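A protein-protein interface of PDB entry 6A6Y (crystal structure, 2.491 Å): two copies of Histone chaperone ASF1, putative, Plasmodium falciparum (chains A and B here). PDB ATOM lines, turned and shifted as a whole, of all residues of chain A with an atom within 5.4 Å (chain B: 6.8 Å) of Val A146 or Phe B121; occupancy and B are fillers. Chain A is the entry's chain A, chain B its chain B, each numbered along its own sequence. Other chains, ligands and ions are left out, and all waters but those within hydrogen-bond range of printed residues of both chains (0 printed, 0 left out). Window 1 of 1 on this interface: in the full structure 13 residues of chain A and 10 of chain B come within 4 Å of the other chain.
The backbone carbonyl oxygen of Glu A147 sits at hydrogen-bond distance from the guanidinium group of Arg B128 (2.6 Å).
OE1 of Glu A147 lies within hydrogen-bond range of ND1 of His B143, 2.7 Å away.
The backbone carbonyl oxygen (O) of Pro A16 is in hydrogen-bond range of the backbone NH (N) of Ile A144.
The backbone carbonyl oxygen (O) of Asn B119 sits at hydrogen-bond distance from the backbone NH (N) of His B143.
The backbone NH of Cys B141 sits at hydrogen-bond distance from the backbone carbonyl oxygen of Phe B121, 2.7 Å away.
Among the printed residues, pairs that only touch across the chains: Glu A147 with Phe B121 (3.4 Å), Pro A16 with Ile B17 (3.6 Å), Val A146 with Ile B17 (3.8 Å), Glu A147 with Asn B119 (3.8 Å), Val A146 with Phe B121 (3.8 Å), Phe A145 with His B143 (3.9 Å) and Pro A149 with Arg B128 (3.9 Å).
Val A146 touches two residues of chain B.
Printed residues of chain A within 4 Å of His B143: Phe A145 (3.9 Å) and Glu A147 (2.7 Å).
Of the printed residues of chain B, Pro A16 touches Ile B17 (3.6 Å).
Of the printed residues of chain B, Glu A147 touches Asn B119 (3.8 Å), Phe B121 (3.4 Å), Arg B128 (2.6 Å) and His B143 (2.7 Å).
Of the printed residues of chain A, Arg B128 touches Glu A147 and Pro A149.
Of the printed residues of chain A, Asn B119 touches Glu A147.
The nearest residue of chain B that does not touch Val A146 is His B143 (4.1 Å).
Of the 17 printed residues of chain B, 5 touch a printed residue of chain A.
Printed residues of chain B that touch a printed residue of chain A: Ile B17, Asn B119, Phe B121, Arg B128 and His B143.
Hydrophobic or aromatic side chains of chain B within 4 Å of the printed part of chain A: Ile B17, Phe B121 and His B143.
Hydrophobic or aromatic side chains of chain A that line the printed part of chain B: Pro A16, Phe A145, Val A146 and Pro A149.
No position is printed for both chains.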
ATOM      1  N   VAL A  13     -31.414 -26.792 -31.306  1.00  0.00           N
ATOM      2  CA  VAL A  13     -32.682 -27.392 -31.712  1.00  0.00           C
ATOM      3  C   VAL A  13     -33.806 -26.518 -31.164  1.00  0.00           C
ATOM      4  O   VAL A  13     -34.093 -26.540 -29.966  1.00  0.00           O
ATOM      5  CB  VAL A  13     -32.811 -28.835 -31.217  1.00  0.00           C
ATOM      6  CG1 VAL A  13     -34.030 -29.492 -31.838  1.00  0.00           C
ATOM      7  CG2 VAL A  13     -31.543 -29.621 -31.534  1.00  0.00           C
ATOM      8  N   PRO A  16     -37.513 -28.534 -29.559  1.00  0.00           N
ATOM      9  CA  PRO A  16     -37.146 -29.937 -29.308  1.00  0.00           C
ATOM     10  C   PRO A  16     -38.320 -30.819 -28.921  1.00  0.00           C
ATOM     11  O   PRO A  16     -38.221 -32.043 -29.061  1.00  0.00           O
ATOM     12  CB  PRO A  16     -36.128 -29.829 -28.164  1.00  0.00           C
ATOM     13  CG  PRO A  16     -36.492 -28.544 -27.474  1.00  0.00           C
ATOM     14  CD  PRO A  16     -36.957 -27.618 -28.549  1.00  0.00           C
ATOM     15  N   TYR A 116     -29.430 -36.280 -33.622  1.00  0.00           N
ATOM     16  CA  TYR A 116     -30.035 -36.344 -32.298  1.00  0.00           C
ATOM     17  C   TYR A 116     -31.115 -37.411 -32.303  1.00  0.00           C
ATOM     18  O   TYR A 116     -31.987 -37.409 -33.177  1.00  0.00           O
ATOM     19  CB  TYR A 116     -30.643 -34.999 -31.888  1.00  0.00           C
ATOM     20  CG  TYR A 116     -29.677 -33.841 -31.903  1.00  0.00           C
ATOM     21  CD1 TYR A 116     -29.469 -33.100 -33.059  1.00  0.00           C
ATOM     22  CD2 TYR A 116     -28.980 -33.481 -30.757  1.00  0.00           C
ATOM     23  CE1 TYR A 116     -28.587 -32.035 -33.077  1.00  0.00           C
ATOM     24  CE2 TYR A 116     -28.099 -32.418 -30.764  1.00  0.00           C
ATOM     25  CZ  TYR A 116     -27.906 -31.699 -31.928  1.00  0.00           C
ATOM     26  OH  TYR A 116     -27.027 -30.641 -31.940  1.00  0.00           O
ATOM     27  N   ILE A 144     -36.870 -34.487 -28.790  1.00  0.00           N
ATOM     28  CA  ILE A 144     -35.499 -34.545 -29.288  1.00  0.00           C
ATOM     29  C   ILE A 144     -34.518 -34.452 -28.125  1.00  0.00           C
ATOM     30  O   ILE A 144     -34.629 -33.561 -27.272  1.00  0.00           O
ATOM     31  CB  ILE A 144     -35.238 -33.430 -30.313  1.00  0.00           C
ATOM     32  CG1 ILE A 144     -36.135 -33.616 -31.538  1.00  0.00           C
ATOM     33  CG2 ILE A 144     -33.767 -33.412 -30.716  1.00  0.00           C
ATOM     34  CD1 ILE A 144     -36.175 -32.416 -32.455  1.00  0.00           C
ATOM     35  N   PHE A 145     -33.558 -35.377 -28.092  1.00  0.00           N
ATOM     36  CA  PHE A 145     -32.593 -35.481 -26.997  1.00  0.00           C
ATOM     37  C   PHE A 145     -31.408 -34.573 -27.284  1.00  0.00           C
ATOM     38  O   PHE A 145     -30.384 -34.990 -27.834  1.00  0.00           O
ATOM     39  CB  PHE A 145     -32.184 -36.930 -26.795  1.00  0.00           C
ATOM     40  CG  PHE A 145     -33.276 -37.752 -26.224  1.00  0.00           C
ATOM     41  CD1 PHE A 145     -34.317 -38.196 -27.022  1.00  0.00           C
ATOM     42  CD2 PHE A 145     -33.308 -38.020 -24.878  1.00  0.00           C
ATOM     43  CE1 PHE A 145     -35.345 -38.928 -26.487  1.00  0.00           C
ATOM     44  CE2 PHE A 145     -34.322 -38.747 -24.349  1.00  0.00           C
ATOM     45  CZ  PHE A 145     -35.349 -39.204 -25.149  1.00  0.00           C
ATOM     46  N   VAL A 146     -31.554 -33.311 -26.883  1.00  0.00           N
ATOM     47  CA  VAL A 146     -30.658 -32.254 -27.319  1.00  0.00           C
ATOM     48  C   VAL A 146     -29.310 -32.323 -26.617  1.00  0.00           C
ATOM     49  O   VAL A 146     -28.335 -31.734 -27.094  1.00  0.00           O
ATOM     50  CB  VAL A 146     -31.339 -30.897 -27.081  1.00  0.00           C
ATOM     51  CG1 VAL A 146     -32.521 -30.729 -28.030  1.00  0.00           C
ATOM     52  CG2 VAL A 146     -31.804 -30.796 -25.636  1.00  0.00           C
ATOM     53  N   GLU A 147     -29.228 -33.041 -25.498  1.00  0.00           N
ATOM     54  CA  GLU A 147     -28.016 -33.090 -24.695  1.00  0.00           C
ATOM     55  C   GLU A 147     -26.980 -34.075 -25.223  1.00  0.00           C
ATOM     56  O   GLU A 147     -25.870 -34.128 -24.681  1.00  0.00           O
ATOM     57  CB  GLU A 147     -28.374 -33.451 -23.250  1.00  0.00           C
ATOM     58  CG  GLU A 147     -28.402 -34.947 -22.947  1.00  0.00           C
ATOM     59  CD  GLU A 147     -29.591 -35.667 -23.567  1.00  0.00           C
ATOM     60  OE1 GLU A 147     -30.486 -34.993 -24.116  1.00  0.00           O
ATOM     61  OE2 GLU A 147     -29.627 -36.917 -23.496  1.00  0.00           O
ATOM     62  N   ASN A 148     -27.298 -34.839 -26.266  1.00  0.00           N
ATOM     63  CA  ASN A 148     -26.474 -35.971 -26.700  1.00  0.00           C
ATOM     64  C   ASN A 148     -26.328 -35.980 -28.219  1.00  0.00           C
ATOM     65  O   ASN A 148     -26.871 -36.851 -28.909  1.00  0.00           O
ATOM     66  CB  ASN A 148     -27.071 -37.285 -26.194  1.00  0.00           C
ATOM     67  CG  ASN A 148     -26.204 -38.481 -26.514  1.00  0.00           C
ATOM     68  OD1 ASN A 148     -24.992 -38.356 -26.674  1.00  0.00           O
ATOM     69  ND2 ASN A 148     -26.825 -39.652 -26.613  1.00  0.00           N
ATOM     70  N   PRO A 149     -25.603 -35.009 -28.780  1.00  0.00           N
ATOM     71  CA  PRO A 149     -25.379 -35.014 -30.233  1.00  0.00           C
ATOM     72  C   PRO A 149     -24.408 -36.114 -30.644  1.00  0.00           C
ATOM     73  O   PRO A 149     -23.406 -36.366 -29.970  1.00  0.00           O
ATOM     74  CB  PRO A 149     -24.798 -33.623 -30.509  1.00  0.00           C
ATOM     75  CG  PRO A 149     -24.165 -33.214 -29.228  1.00  0.00           C
ATOM     76  CD  PRO A 149     -24.954 -33.861 -28.120  1.00  0.00           C
ATOM     77  N   ILE B  17     -36.538 -27.825 -21.412  1.00  0.00           N
ATOM     78  CA  ILE B  17     -35.256 -27.568 -22.053  1.00  0.00           C
ATOM     79  C   ILE B  17     -35.072 -26.059 -22.152  1.00  0.00           C
ATOM     80  O   ILE B  17     -35.794 -25.389 -22.901  1.00  0.00           O
ATOM     81  CB  ILE B  17     -35.169 -28.233 -23.432  1.00  0.00           C
ATOM     82  CG1 ILE B  17     -35.493 -29.731 -23.309  1.00  0.00           C
ATOM     83  CG2 ILE B  17     -33.792 -28.083 -23.977  1.00  0.00           C
ATOM     84  CD1 ILE B  17     -35.418 -30.505 -24.606  1.00  0.00           C
ATOM     85  N   ILE B  20     -30.095 -22.735 -17.804  1.00  0.00           N
ATOM     86  CA  ILE B  20     -30.184 -23.108 -16.395  1.00  0.00           C
ATOM     87  C   ILE B  20     -30.528 -21.921 -15.505  1.00  0.00           C
ATOM     88  O   ILE B  20     -31.000 -22.116 -14.379  1.00  0.00           O
ATOM     89  CB  ILE B  20     -28.880 -23.772 -15.912  1.00  0.00           C
ATOM     90  CG1 ILE B  20     -27.691 -22.830 -16.106  1.00  0.00           C
ATOM     91  CG2 ILE B  20     -28.655 -25.101 -16.628  1.00  0.00           C
ATOM     92  CD1 ILE B  20     -26.444 -23.264 -15.363  1.00  0.00           C
ATOM     93  N   VAL B  94     -23.603 -28.496 -11.213  1.00  0.00           N
ATOM     94  CA  VAL B  94     -24.135 -27.579 -12.214  1.00  0.00           C
ATOM     95  C   VAL B  94     -24.160 -28.222 -13.595  1.00  0.00           C
ATOM     96  O   VAL B  94     -25.204 -28.265 -14.253  1.00  0.00           O
ATOM     97  CB  VAL B  94     -23.337 -26.256 -12.245  1.00  0.00           C
ATOM     98  CG1 VAL B  94     -23.910 -25.313 -13.290  1.00  0.00           C
ATOM     99  CG2 VAL B  94     -23.329 -25.604 -10.870  1.00  0.00           C
ATOM    100  N   LEU B  95     -23.018 -28.729 -14.048  1.00  0.00           N
ATOM    101  CA  LEU B  95     -22.914 -29.445 -15.310  1.00  0.00           C
ATOM    102  C   LEU B  95     -22.997 -30.942 -15.054  1.00  0.00           C
ATOM    103  O   LEU B  95     -22.374 -31.456 -14.121  1.00  0.00           O
ATOM    104  CB  LEU B  95     -21.596 -29.125 -16.019  1.00  0.00           C
ATOM    105  CG  LEU B  95     -21.460 -27.808 -16.782  1.00  0.00           C
ATOM    106  CD1 LEU B  95     -19.991 -27.473 -16.979  1.00  0.00           C
ATOM    107  CD2 LEU B  95     -22.177 -27.884 -18.120  1.00  0.00           C
ATOM    108  N   GLY B  96     -23.780 -31.636 -15.873  1.00  0.00           N
ATOM    109  CA  GLY B  96     -23.898 -33.071 -15.721  1.00  0.00           C
ATOM    110  C   GLY B  96     -25.289 -33.528 -15.345  1.00  0.00           C
ATOM    111  O   GLY B  96     -26.273 -32.820 -15.585  1.00  0.00           O
ATOM    112  N   ASN B 119     -30.017 -33.421 -17.572  1.00  0.00           N
ATOM    113  CA  ASN B 119     -28.653 -33.184 -18.018  1.00  0.00           C
ATOM    114  C   ASN B 119     -28.463 -31.698 -18.300  1.00  0.00           C
ATOM    115  O   ASN B 119     -29.298 -31.076 -18.965  1.00  0.00           O
ATOM    116  CB  ASN B 119     -28.332 -34.003 -19.267  1.00  0.00           C
ATOM    117  CG  ASN B 119     -26.843 -34.136 -19.505  1.00  0.00           C
ATOM    118  OD1 ASN B 119     -26.215 -33.258 -20.098  1.00  0.00           O
ATOM    119  ND2 ASN B 119     -26.268 -35.237 -19.040  1.00  0.00           N
ATOM    120  N   SER B 120     -27.366 -31.138 -17.802  1.00  0.00           N
ATOM    121  CA  SER B 120     -27.008 -29.745 -18.032  1.00  0.00           C
ATOM    122  C   SER B 120     -25.686 -29.703 -18.784  1.00  0.00           C
ATOM    123  O   SER B 120     -24.734 -30.395 -18.410  1.00  0.00           O
ATOM    124  CB  SER B 120     -26.912 -28.970 -16.717  1.00  0.00           C
ATOM    125  OG  SER B 120     -28.175 -28.908 -16.080  1.00  0.00           O
ATOM    126  N   PHE B 121     -25.622 -28.881 -19.828  1.00  0.00           N
ATOM    127  CA  PHE B 121     -24.495 -28.932 -20.747  1.00  0.00           C
ATOM    128  C   PHE B 121     -24.314 -27.581 -21.420  1.00  0.00           C
ATOM    129  O   PHE B 121     -25.268 -26.815 -21.572  1.00  0.00           O
ATOM    130  CB  PHE B 121     -24.718 -30.011 -21.814  1.00  0.00           C
ATOM    131  CG  PHE B 121     -26.020 -29.859 -22.554  1.00  0.00           C
ATOM    132  CD1 PHE B 121     -27.217 -30.264 -21.979  1.00  0.00           C
ATOM    133  CD2 PHE B 121     -26.050 -29.293 -23.819  1.00  0.00           C
ATOM    134  CE1 PHE B 121     -28.417 -30.106 -22.654  1.00  0.00           C
ATOM    135  CE2 PHE B 121     -27.245 -29.140 -24.500  1.00  0.00           C
ATOM    136  CZ  PHE B 121     -28.429 -29.548 -23.919  1.00  0.00           C
ATOM    137  N   TYR B 122     -23.078 -27.304 -21.828  1.00  0.00           N
ATOM    138  CA  TYR B 122     -22.794 -26.103 -22.600  1.00  0.00           C
ATOM    139  C   TYR B 122     -23.461 -26.165 -23.969  1.00  0.00           C
ATOM    140  O   TYR B 122     -23.440 -27.200 -24.645  1.00  0.00           O
ATOM    141  CB  TYR B 122     -21.285 -25.917 -22.762  1.00  0.00           C
ATOM    142  CG  TYR B 122     -20.625 -25.236 -21.583  1.00  0.00           C
ATOM    143  CD1 TYR B 122     -20.837 -23.886 -21.328  1.00  0.00           C
ATOM    144  CD2 TYR B 122     -19.788 -25.941 -20.727  1.00  0.00           C
ATOM    145  CE1 TYR B 122     -20.238 -23.256 -20.253  1.00  0.00           C
ATOM    146  CE2 TYR B 122     -19.182 -25.320 -19.647  1.00  0.00           C
ATOM    147  CZ  TYR B 122     -19.411 -23.977 -19.415  1.00  0.00           C
ATOM    148  OH  TYR B 122     -18.812 -23.356 -18.343  1.00  0.00           O
ATOM    149  N   LYS B 123     -24.061 -25.045 -24.374  1.00  0.00           N
ATOM    150  CA  LYS B 123     -24.704 -24.952 -25.680  1.00  0.00           C
ATOM    151  C   LYS B 123     -23.683 -24.827 -26.803  1.00  0.00           C
ATOM    152  O   LYS B 123     -23.936 -25.289 -27.922  1.00  0.00           O
ATOM    153  CB  LYS B 123     -25.674 -23.774 -25.705  1.00  0.00           C
ATOM    154  CG  LYS B 123     -26.665 -23.795 -24.556  1.00  0.00           C
ATOM    155  CD  LYS B 123     -27.668 -22.667 -24.669  1.00  0.00           C
ATOM    156  CE  LYS B 123     -27.087 -21.355 -24.181  1.00  0.00           C
ATOM    157  NZ  LYS B 123     -28.119 -20.282 -24.156  1.00  0.00           N
ATOM    158  N   ASP B 124     -22.545 -24.198 -26.528  1.00  0.00           N
ATOM    159  CA  ASP B 124     -21.491 -24.023 -27.516  1.00  0.00           C
ATOM    160  C   ASP B 124     -20.580 -25.246 -27.511  1.00  0.00           C
ATOM    161  O   ASP B 124     -20.176 -25.724 -26.447  1.00  0.00           O
ATOM    162  CB  ASP B 124     -20.688 -22.757 -27.214  1.00  0.00           C
ATOM    163  CG  ASP B 124     -19.497 -22.588 -28.133  1.00  0.00           C
ATOM    164  OD1 ASP B 124     -19.661 -22.029 -29.239  1.00  0.00           O
ATOM    165  OD2 ASP B 124     -18.392 -23.016 -27.745  1.00  0.00           O
ATOM    166  N   ARG B 128     -18.160 -27.044 -24.686  1.00  0.00           N
ATOM    167  CA  ARG B 128     -18.461 -28.419 -24.297  1.00  0.00           C
ATOM    168  C   ARG B 128     -17.202 -29.277 -24.313  1.00  0.00           C
ATOM    169  O   ARG B 128     -16.945 -30.042 -23.377  1.00  0.00           O
ATOM    170  CB  ARG B 128     -19.530 -29.017 -25.210  1.00  0.00           C
ATOM    171  CG  ARG B 128     -20.338 -30.106 -24.520  1.00  0.00           C
ATOM    172  CD  ARG B 128     -21.138 -30.976 -25.478  1.00  0.00           C
ATOM    173  NE  ARG B 128     -21.744 -32.102 -24.767  1.00  0.00           N
ATOM    174  CZ  ARG B 128     -23.052 -32.310 -24.657  1.00  0.00           C
ATOM    175  NH1 ARG B 128     -23.911 -31.475 -25.228  1.00  0.00           N
ATOM    176  NH2 ARG B 128     -23.503 -33.360 -23.982  1.00  0.00           N
ATOM    177  N   LYS B 139     -24.344 -19.735 -20.717  1.00  0.00           N
ATOM    178  CA  LYS B 139     -24.224 -20.571 -21.904  1.00  0.00           C
ATOM    179  C   LYS B 139     -24.403 -22.054 -21.592  1.00  0.00           C
ATOM    180  O   LYS B 139     -23.988 -22.907 -22.382  1.00  0.00           O
ATOM    181  CB  LYS B 139     -22.878 -20.314 -22.581  1.00  0.00           C
ATOM    182  CG  LYS B 139     -22.575 -18.829 -22.728  1.00  0.00           C
ATOM    183  CD  LYS B 139     -21.441 -18.569 -23.701  1.00  0.00           C
ATOM    184  CE  LYS B 139     -21.162 -17.080 -23.824  1.00  0.00           C
ATOM    185  NZ  LYS B 139     -20.904 -16.439 -22.503  1.00  0.00           N
ATOM    186  N   ILE B 140     -25.012 -22.376 -20.454  1.00  0.00           N
ATOM    187  CA  ILE B 140     -25.307 -23.751 -20.069  1.00  0.00           C
ATOM    188  C   ILE B 140     -26.810 -23.957 -20.175  1.00  0.00           C
ATOM    189  O   ILE B 140     -27.595 -23.076 -19.803  1.00  0.00           O
ATOM    190  CB  ILE B 140     -24.805 -24.070 -18.644  1.00  0.00           C
ATOM    191  CG1 ILE B 140     -23.291 -23.883 -18.555  1.00  0.00           C
ATOM    192  CG2 ILE B 140     -25.184 -25.491 -18.235  1.00  0.00           C
ATOM    193  CD1 ILE B 140     -22.755 -23.943 -17.145  1.00  0.00           C
ATOM    194  N   CYS B 141     -27.209 -25.121 -20.676  1.00  0.00           N
ATOM    195  CA  CYS B 141     -28.612 -25.455 -20.845  1.00  0.00           C
ATOM    196  C   CYS B 141     -28.914 -26.758 -20.121  1.00  0.00           C
ATOM    197  O   CYS B 141     -28.071 -27.653 -20.046  1.00  0.00           O
ATOM    198  CB  CYS B 141     -28.962 -25.581 -22.332  1.00  0.00           C
ATOM    199  SG  CYS B 141     -30.611 -26.209 -22.661  1.00  0.00           S
ATOM    200  N   ARG B 142     -30.129 -26.863 -19.592  1.00  0.00           N
ATOM    201  CA  ARG B 142     -30.582 -28.076 -18.932  1.00  0.00           C
ATOM    202  C   ARG B 142     -31.649 -28.760 -19.771  1.00  0.00           C
ATOM    203  O   ARG B 142     -32.452 -28.106 -20.443  1.00  0.00           O
ATOM    204  CB  ARG B 142     -31.123 -27.786 -17.525  1.00  0.00           C
ATOM    205  CG  ARG B 142     -32.450 -27.043 -17.486  1.00  0.00           C
ATOM    206  CD  ARG B 142     -33.017 -27.001 -16.072  1.00  0.00           C
ATOM    207  NE  ARG B 142     -34.108 -26.038 -15.962  1.00  0.00           N
ATOM    208  CZ  ARG B 142     -33.987 -24.828 -15.425  1.00  0.00           C
ATOM    209  NH1 ARG B 142     -32.820 -24.434 -14.932  1.00  0.00           N
ATOM    210  NH2 ARG B 142     -35.031 -24.013 -15.376  1.00  0.00           N
ATOM    211  N   HIS B 143     -31.642 -30.088 -19.734  1.00  0.00           N
ATOM    212  CA  HIS B 143     -32.642 -30.911 -20.404  1.00  0.00           C
ATOM    213  C   HIS B 143     -33.278 -31.801 -19.349  1.00  0.00           C
ATOM    214  O   HIS B 143     -32.646 -32.744 -18.864  1.00  0.00           O
ATOM    215  CB  HIS B 143     -32.021 -31.741 -21.528  1.00  0.00           C
ATOM    216  CG  HIS B 143     -32.967 -32.721 -22.155  1.00  0.00           C
ATOM    217  ND1 HIS B 143     -32.539 -33.785 -22.919  1.00  0.00           N
ATOM    218  CD2 HIS B 143     -34.319 -32.796 -22.133  1.00  0.00           C
ATOM    219  CE1 HIS B 143     -33.585 -34.473 -23.340  1.00  0.00           C
ATOM    220  NE2 HIS B 143     -34.677 -33.895 -22.876  1.00  0.00           N
